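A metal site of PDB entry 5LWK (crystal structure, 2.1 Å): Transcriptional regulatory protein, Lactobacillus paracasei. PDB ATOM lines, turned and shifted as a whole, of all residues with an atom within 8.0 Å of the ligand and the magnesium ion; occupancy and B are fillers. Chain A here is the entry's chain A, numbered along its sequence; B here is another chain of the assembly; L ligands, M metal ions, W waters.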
ATOM      1  N   VAL A   7      18.128  26.497 -32.512  1.00  0.00           N
ATOM      2  CA  VAL A   7      18.798  25.274 -32.903  1.00  0.00           C
ATOM      3  C   VAL A   7      17.807  24.148 -32.726  1.00  0.00           C
ATOM      4  O   VAL A   7      17.517  23.753 -31.642  1.00  0.00           O
ATOM      5  CB  VAL A   7      19.992  25.018 -32.012  1.00  0.00           C
ATOM      6  CG1 VAL A   7      20.769  23.804 -32.464  1.00  0.00           C
ATOM      7  CG2 VAL A   7      20.880  26.232 -31.938  1.00  0.00           C
ATOM      8  N   GLU A   8      17.274  23.686 -33.828  1.00  0.00           N
ATOM      9  CA  GLU A   8      16.300  22.632 -33.816  1.00  0.00           C
ATOM     10  C   GLU A   8      16.308  21.967 -35.179  1.00  0.00           C
ATOM     11  O   GLU A   8      16.347  22.640 -36.184  1.00  0.00           O
ATOM     12  CB  GLU A   8      14.945  23.236 -33.513  1.00  0.00           C
ATOM     13  CG  GLU A   8      13.740  22.523 -34.058  1.00  0.00           C
ATOM     14  CD  GLU A   8      13.401  21.293 -33.272  1.00  0.00           C
ATOM     15  OE1 GLU A   8      13.195  21.375 -32.077  1.00  0.00           O
ATOM     16  OE2 GLU A   8      13.357  20.241 -33.866  1.00  0.00           O
ATOM     17  N   ASP A   9      16.306  20.657 -35.198  1.00  0.00           N
ATOM     18  CA  ASP A   9      16.290  19.890 -36.425  1.00  0.00           C
ATOM     19  C   ASP A   9      15.012  19.858 -37.261  1.00  0.00           C
ATOM     20  O   ASP A   9      15.054  19.823 -38.451  1.00  0.00           O
ATOM     21  CB  ASP A   9      16.921  18.524 -36.226  1.00  0.00           C
ATOM     22  CG  ASP A   9      16.188  17.681 -35.248  1.00  0.00           C
ATOM     23  OD1 ASP A   9      16.072  18.011 -34.088  1.00  0.00           O
ATOM     24  OD2 ASP A   9      15.745  16.633 -35.651  1.00  0.00           O
ATOM     25  N   ASP A  10      13.877  19.830 -36.613  1.00  0.00           N
ATOM     26  CA  ASP A  10      12.584  19.746 -37.295  1.00  0.00           C
ATOM     27  C   ASP A  10      12.189  21.107 -37.890  1.00  0.00           C
ATOM     28  O   ASP A  10      11.986  22.054 -37.138  1.00  0.00           O
ATOM     29  CB  ASP A  10      11.490  19.247 -36.339  1.00  0.00           C
ATOM     30  CG  ASP A  10      10.219  18.852 -37.077  1.00  0.00           C
ATOM     31  OD1 ASP A  10       9.456  19.745 -37.493  1.00  0.00           O
ATOM     32  OD2 ASP A  10       9.994  17.644 -37.267  1.00  0.00           O
ATOM     33  N   VAL A  13       8.991  22.705 -36.480  1.00  0.00           N
ATOM     34  CA  VAL A  13       9.210  23.290 -35.148  1.00  0.00           C
ATOM     35  C   VAL A  13       9.976  24.608 -35.256  1.00  0.00           C
ATOM     36  O   VAL A  13       9.680  25.560 -34.524  1.00  0.00           O
ATOM     37  CB  VAL A  13       9.910  22.308 -34.180  1.00  0.00           C
ATOM     38  CG1 VAL A  13      10.114  22.958 -32.808  1.00  0.00           C
ATOM     39  CG2 VAL A  13       9.077  21.044 -34.017  1.00  0.00           C
ATOM     40  N   GLU A  34      19.850  23.897 -38.023  1.00  0.00           N
ATOM     41  CA  GLU A  34      19.353  22.538 -37.801  1.00  0.00           C
ATOM     42  C   GLU A  34      20.390  21.629 -37.160  1.00  0.00           C
ATOM     43  O   GLU A  34      20.049  20.526 -36.728  1.00  0.00           O
ATOM     44  CB  GLU A  34      18.859  21.949 -39.125  1.00  0.00           C
ATOM     45  CG  GLU A  34      17.846  22.852 -39.818  1.00  0.00           C
ATOM     46  CD  GLU A  34      17.011  22.147 -40.884  1.00  0.00           C
ATOM     47  OE1 GLU A  34      15.910  22.675 -41.187  1.00  0.00           O
ATOM     48  OE2 GLU A  34      17.442  21.100 -41.415  1.00  0.00           O
ATOM     49  N   LEU A  53      17.291  26.030 -27.692  1.00  0.00           N
ATOM     50  CA  LEU A  53      17.967  24.788 -27.992  1.00  0.00           C
ATOM     51  C   LEU A  53      17.228  23.468 -27.807  1.00  0.00           C
ATOM     52  O   LEU A  53      16.739  23.176 -26.765  1.00  0.00           O
ATOM     53  CB  LEU A  53      19.246  24.769 -27.165  1.00  0.00           C
ATOM     54  CG  LEU A  53      20.260  23.653 -27.242  1.00  0.00           C
ATOM     55  CD1 LEU A  53      20.877  23.565 -28.609  1.00  0.00           C
ATOM     56  CD2 LEU A  53      21.324  23.861 -26.197  1.00  0.00           C
ATOM     57  N   ASP A  54      17.186  22.692 -28.870  1.00  0.00           N
ATOM     58  CA  ASP A  54      16.612  21.377 -28.892  1.00  0.00           C
ATOM     59  C   ASP A  54      17.709  20.482 -28.389  1.00  0.00           C
ATOM     60  O   ASP A  54      18.838  20.882 -28.391  1.00  0.00           O
ATOM     61  CB  ASP A  54      16.231  21.028 -30.313  1.00  0.00           C
ATOM     62  CG  ASP A  54      15.595  19.658 -30.449  1.00  0.00           C
ATOM     63  OD1 ASP A  54      14.980  19.169 -29.521  1.00  0.00           O
ATOM     64  OD2 ASP A  54      15.708  19.079 -31.522  1.00  0.00           O
ATOM     65  N   ILE A  55      17.388  19.297 -27.927  1.00  0.00           N
ATOM     66  CA  ILE A  55      18.408  18.323 -27.454  1.00  0.00           C
ATOM     67  C   ILE A  55      18.801  17.300 -28.535  1.00  0.00           C
ATOM     68  O   ILE A  55      19.990  17.140 -28.812  1.00  0.00           O
ATOM     69  CB  ILE A  55      17.996  17.622 -26.149  1.00  0.00           C
ATOM     70  CG1 ILE A  55      18.017  18.639 -24.999  1.00  0.00           C
ATOM     71  CG2 ILE A  55      18.938  16.462 -25.835  1.00  0.00           C
ATOM     72  CD1 ILE A  55      17.554  18.100 -23.663  1.00  0.00           C
ATOM     73  N   ARG A  56      17.829  16.597 -29.115  1.00  0.00           N
ATOM     74  CA  ARG A  56      18.131  15.622 -30.168  1.00  0.00           C
ATOM     75  C   ARG A  56      18.276  16.335 -31.506  1.00  0.00           C
ATOM     76  O   ARG A  56      17.291  16.699 -32.119  1.00  0.00           O
ATOM     77  CB  ARG A  56      17.049  14.550 -30.285  1.00  0.00           C
ATOM     78  CG  ARG A  56      17.045  13.499 -29.195  1.00  0.00           C
ATOM     79  CD  ARG A  56      16.931  12.094 -29.784  1.00  0.00           C
ATOM     80  NE  ARG A  56      15.750  11.942 -30.657  1.00  0.00           N
ATOM     81  CZ  ARG A  56      15.693  11.236 -31.791  1.00  0.00           C
ATOM     82  NH1 ARG A  56      16.755  10.572 -32.274  1.00  0.00           N
ATOM     83  NH2 ARG A  56      14.549  11.198 -32.479  1.00  0.00           N
ATOM     84  N   LEU A  57      19.521  16.525 -31.937  1.00  0.00           N
ATOM     85  CA  LEU A  57      19.808  17.052 -33.275  1.00  0.00           C
ATOM     86  C   LEU A  57      20.348  15.933 -34.138  1.00  0.00           C
ATOM     87  O   LEU A  57      20.679  14.852 -33.644  1.00  0.00           O
ATOM     88  CB  LEU A  57      20.828  18.204 -33.204  1.00  0.00           C
ATOM     89  CG  LEU A  57      20.372  19.561 -32.627  1.00  0.00           C
ATOM     90  CD1 LEU A  57      18.997  19.974 -33.141  1.00  0.00           C
ATOM     91  CD2 LEU A  57      20.396  19.557 -31.111  1.00  0.00           C
ATOM     92  N   LYS A  58      20.420  16.193 -35.438  1.00  0.00           N
ATOM     93  CA  LYS A  58      20.952  15.203 -36.394  1.00  0.00           C
ATOM     94  C   LYS A  58      22.428  14.906 -36.103  1.00  0.00           C
ATOM     95  O   LYS A  58      22.809  13.741 -35.994  1.00  0.00           O
ATOM     96  CB  LYS A  58      20.776  15.693 -37.825  1.00  0.00           C
ATOM     97  N   GLY A  60      24.323  15.612 -33.355  1.00  0.00           N
ATOM     98  CA  GLY A  60      24.747  15.455 -31.966  1.00  0.00           C
ATOM     99  C   GLY A  60      23.684  15.877 -30.954  1.00  0.00           C
ATOM    100  O   GLY A  60      22.525  16.037 -31.304  1.00  0.00           O
ATOM    101  N   ASN A  61      24.121  16.066 -29.716  1.00  0.00           N
ATOM    102  CA  ASN A  61      23.233  16.251 -28.585  1.00  0.00           C
ATOM    103  C   ASN A  61      23.359  17.664 -27.997  1.00  0.00           C
ATOM    104  O   ASN A  61      24.455  18.112 -27.676  1.00  0.00           O
ATOM    105  CB  ASN A  61      23.548  15.184 -27.546  1.00  0.00           C
ATOM    106  CG  ASN A  61      22.661  15.270 -26.333  1.00  0.00           C
ATOM    107  OD1 ASN A  61      22.842  16.146 -25.487  1.00  0.00           O
ATOM    108  ND2 ASN A  61      21.688  14.352 -26.224  1.00  0.00           N
ATOM    109  N   GLY A  62      22.225  18.327 -27.828  1.00  0.00           N
ATOM    110  CA  GLY A  62      22.172  19.686 -27.312  1.00  0.00           C
ATOM    111  C   GLY A  62      22.715  19.925 -25.914  1.00  0.00           C
ATOM    112  O   GLY A  62      23.092  21.052 -25.596  1.00  0.00           O
ATOM    113  N   LEU A  80      15.943  25.656 -23.164  1.00  0.00           N
ATOM    114  CA  LEU A  80      15.856  24.368 -23.779  1.00  0.00           C
ATOM    115  C   LEU A  80      14.417  24.077 -24.129  1.00  0.00           C
ATOM    116  O   LEU A  80      13.559  24.203 -23.312  1.00  0.00           O
ATOM    117  CB  LEU A  80      16.376  23.303 -22.841  1.00  0.00           C
ATOM    118  CG  LEU A  80      17.862  23.132 -22.665  1.00  0.00           C
ATOM    119  CD1 LEU A  80      18.178  22.327 -21.442  1.00  0.00           C
ATOM    120  CD2 LEU A  80      18.505  22.519 -23.882  1.00  0.00           C
ATOM    121  N   ILE A  81      14.163  23.715 -25.372  1.00  0.00           N
ATOM    122  CA  ILE A  81      12.831  23.350 -25.853  1.00  0.00           C
ATOM    123  C   ILE A  81      13.037  21.983 -26.455  1.00  0.00           C
ATOM    124  O   ILE A  81      13.662  21.857 -27.470  1.00  0.00           O
ATOM    125  CB  ILE A  81      12.299  24.332 -26.878  1.00  0.00           C
ATOM    126  CG1 ILE A  81      12.382  25.741 -26.306  1.00  0.00           C
ATOM    127  CG2 ILE A  81      10.872  23.989 -27.219  1.00  0.00           C
ATOM    128  CD1 ILE A  81      11.708  26.786 -27.117  1.00  0.00           C
ATOM    129  N   THR A  82      12.507  20.961 -25.805  1.00  0.00           N
ATOM    130  CA  THR A  82      12.768  19.622 -26.212  1.00  0.00           C
ATOM    131  C   THR A  82      11.739  18.628 -25.713  1.00  0.00           C
ATOM    132  O   THR A  82      10.968  18.934 -24.849  1.00  0.00           O
ATOM    133  CB  THR A  82      14.125  19.236 -25.616  1.00  0.00           C
ATOM    134  OG1 THR A  82      14.488  17.933 -25.984  1.00  0.00           O
ATOM    135  CG2 THR A  82      14.066  19.315 -24.154  1.00  0.00           C
ATOM    136  N   ALA A  83      11.755  17.445 -26.291  1.00  0.00           N
ATOM    137  CA  ALA A  83      10.891  16.366 -25.937  1.00  0.00           C
ATOM    138  C   ALA A  83      11.479  15.541 -24.821  1.00  0.00           C
ATOM    139  O   ALA A  83      10.799  14.745 -24.221  1.00  0.00           O
ATOM    140  CB  ALA A  83      10.656  15.495 -27.140  1.00  0.00           C
ATOM    141  N   ALA A  84      12.743  15.746 -24.551  1.00  0.00           N
ATOM    142  CA  ALA A  84      13.438  14.959 -23.557  1.00  0.00           C
ATOM    143  C   ALA A  84      12.949  15.047 -22.133  1.00  0.00           C
ATOM    144  O   ALA A  84      12.700  16.094 -21.609  1.00  0.00           O
ATOM    145  CB  ALA A  84      14.915  15.278 -23.603  1.00  0.00           C
ATOM    146  N   ASN A  85      12.822  13.896 -21.510  1.00  0.00           N
ATOM    147  CA  ASN A  85      12.425  13.775 -20.130  1.00  0.00           C
ATOM    148  C   ASN A  85      13.672  13.456 -19.313  1.00  0.00           C
ATOM    149  O   ASN A  85      14.742  13.458 -19.853  1.00  0.00           O
ATOM    150  CB  ASN A  85      11.279  12.798 -19.922  1.00  0.00           C
ATOM    151  CG  ASN A  85      11.662  11.383 -20.199  1.00  0.00           C
ATOM    152  OD1 ASN A  85      12.775  11.084 -20.485  1.00  0.00           O
ATOM    153  ND2 ASN A  85      10.703  10.512 -20.132  1.00  0.00           N
ATOM    154  N   ASN A  88      15.766  10.479 -20.521  1.00  0.00           N
ATOM    155  CA  ASN A  88      16.384  10.751 -21.786  1.00  0.00           C
ATOM    156  C   ASN A  88      17.680  11.518 -21.542  1.00  0.00           C
ATOM    157  O   ASN A  88      18.665  11.247 -22.158  1.00  0.00           O
ATOM    158  CB  ASN A  88      15.463  11.549 -22.707  1.00  0.00           C
ATOM    159  CG  ASN A  88      14.224  10.796 -23.117  1.00  0.00           C
ATOM    160  OD1 ASN A  88      14.231   9.602 -23.251  1.00  0.00           O
ATOM    161  ND2 ASN A  88      13.166  11.523 -23.329  1.00  0.00           N
ATOM    162  N   TYR B 101      13.115  25.388 -19.153  1.00  0.00           N
ATOM    163  CA  TYR B 101      13.099  24.136 -19.836  1.00  0.00           C
ATOM    164  C   TYR B 101      11.691  23.846 -20.291  1.00  0.00           C
ATOM    165  O   TYR B 101      10.858  23.531 -19.486  1.00  0.00           O
ATOM    166  CB  TYR B 101      13.594  23.045 -18.895  1.00  0.00           C
ATOM    167  CG  TYR B 101      13.885  21.703 -19.517  1.00  0.00           C
ATOM    168  CD1 TYR B 101      12.878  20.853 -19.878  1.00  0.00           C
ATOM    169  CD2 TYR B 101      15.173  21.288 -19.687  1.00  0.00           C
ATOM    170  CE1 TYR B 101      13.157  19.637 -20.431  1.00  0.00           C
ATOM    171  CE2 TYR B 101      15.442  20.074 -20.229  1.00  0.00           C
ATOM    172  CZ  TYR B 101      14.431  19.255 -20.591  1.00  0.00           C
ATOM    173  OH  TYR B 101      14.705  18.061 -21.123  1.00  0.00           O
ATOM    174  N   LEU B 102      11.439  23.938 -21.584  1.00  0.00           N
ATOM    175  CA  LEU B 102      10.109  23.701 -22.159  1.00  0.00           C
ATOM    176  C   LEU B 102      10.021  22.314 -22.721  1.00  0.00           C
ATOM    177  O   LEU B 102      10.769  21.959 -23.632  1.00  0.00           O
ATOM    178  CB  LEU B 102       9.780  24.675 -23.284  1.00  0.00           C
ATOM    179  CG  LEU B 102       9.002  25.889 -22.842  1.00  0.00           C
ATOM    180  CD1 LEU B 102       9.876  26.742 -21.955  1.00  0.00           C
ATOM    181  CD2 LEU B 102       8.507  26.664 -24.057  1.00  0.00           C
ATOM    182  N   ILE B 103       9.084  21.548 -22.196  1.00  0.00           N
ATOM    183  CA  ILE B 103       8.828  20.211 -22.682  1.00  0.00           C
ATOM    184  C   ILE B 103       7.870  20.345 -23.866  1.00  0.00           C
ATOM    185  O   ILE B 103       6.857  21.046 -23.780  1.00  0.00           O
ATOM    186  CB  ILE B 103       8.212  19.324 -21.574  1.00  0.00           C
ATOM    187  CG1 ILE B 103       9.163  19.254 -20.371  1.00  0.00           C
ATOM    188  CG2 ILE B 103       7.963  17.915 -22.079  1.00  0.00           C
ATOM    189  CD1 ILE B 103       8.470  18.935 -19.068  1.00  0.00           C
ATOM    190  N   LYS B 104       8.215  19.715 -24.982  1.00  0.00           N
ATOM    191  CA  LYS B 104       7.291  19.601 -26.112  1.00  0.00           C
ATOM    192  C   LYS B 104       6.223  18.567 -25.729  1.00  0.00           C
ATOM    193  O   LYS B 104       6.586  17.524 -25.189  1.00  0.00           O
ATOM    194  CB  LYS B 104       8.023  19.113 -27.371  1.00  0.00           C
ATOM    195  CG  LYS B 104       9.081  20.060 -27.912  1.00  0.00           C
ATOM    196  CD  LYS B 104       9.843  19.370 -29.028  1.00  0.00           C
ATOM    197  CE  LYS B 104      10.875  20.278 -29.666  1.00  0.00           C
ATOM    198  NZ  LYS B 104      11.721  19.509 -30.618  1.00  0.00           N
HETATM  199 BE1  LIG L   1      14.424  17.490 -29.446  1.00  0.00          BE
HETATM  200  F1  LIG L   1      14.622  16.657 -30.663  1.00  0.00           F
HETATM  201  F2  LIG L   1      12.936  17.545 -29.227  1.00  0.00           F
HETATM  202  F3  LIG L   1      15.209  17.154 -28.210  1.00  0.00           F
HETATM  203 MG    MG M   1      15.333  17.199 -32.386  1.00  0.00          MG
HETATM  204  O   HOH W   1      14.997  15.387 -33.174  1.00  0.00           O
HETATM  205  O   HOH W   2      13.468  17.826 -32.655  1.00  0.00           O
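A fluorine (F3) of the ligand sits at hydrogen-bond distance from the backbone NH of Arg 56. The side-chain amino group of Lys 104 of chain B sits at hydrogen-bond distance from a fluorine (F2) of the ligand (2.7 Å). N of Ala 83 sits at hydrogen-bond distance from F2 of the ligand, 3.2 Å away. A beryllium atom (BE1) of the ligand is bound by the side-chain carboxylate (OD1) of Asp 54 (1.8 Å). F3 of the ligand lies within hydrogen-bond range of OG1 of Thr 82, at 2.5 Å. A fluorine (F3) of the ligand lies within hydrogen-bond range of the backbone NH of Ile 55, 3.1 Å away.
N of Gly 62 lies within hydrogen-bond range of O of Ile 55 (2.7 Å). The side-chain amino group (NZ) of Lys 104 of chain B sits close to the side-chain carboxylate (OD1) of Asp 54, at 3.5 Å. N of Asp 54 lies within hydrogen-bond range of O of Val 7, at 3.0 Å. NZ of Lys 104 of chain B lies within salt-bridge range of OE1 of Glu 8, 2.8 Å away. The backbone NH of Thr 82 lies within hydrogen-bond range of the backbone carbonyl oxygen of Leu 102 of chain B (3.0 Å). The backbone carbonyl oxygen of Thr 82 lies within hydrogen-bond range of the backbone NH of Lys 104 of chain B (2.9 Å). OE2 of Glu 8 is in hydrogen-bond range of N of Asp 10 (2.8 Å). The side-chain hydroxyl (OG1) of Thr 82 sits at hydrogen-bond distance from the backbone NH (N) of Ala 84.
Within 4 Å of the ligand: Asp 9, Asp 54, Ile 55, Arg 56, Thr 82, Ala 83 and Lys 104 of chain B. The nearest printed residue that does not touch the ligand is Ala 84 (4.6 Å).
Merely in contact with the magnesium ion: Glu 8. Four residues have an atom within 4 Å of the magnesium ion: Glu 8, Asp 9, Asp 54 and Arg 56.
The magnesium ion is bound by F1 of the ligand, water W2, water W1, OD1 of Asp 9, O of Arg 56 and OD2 of Asp 54. The magnesium ion has six donor atoms within binding distance.
Water W2 bridges the side-chain carboxylate (OE2) of Glu 8 and the side-chain amino group (NZ) of Lys 104 of chain B.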
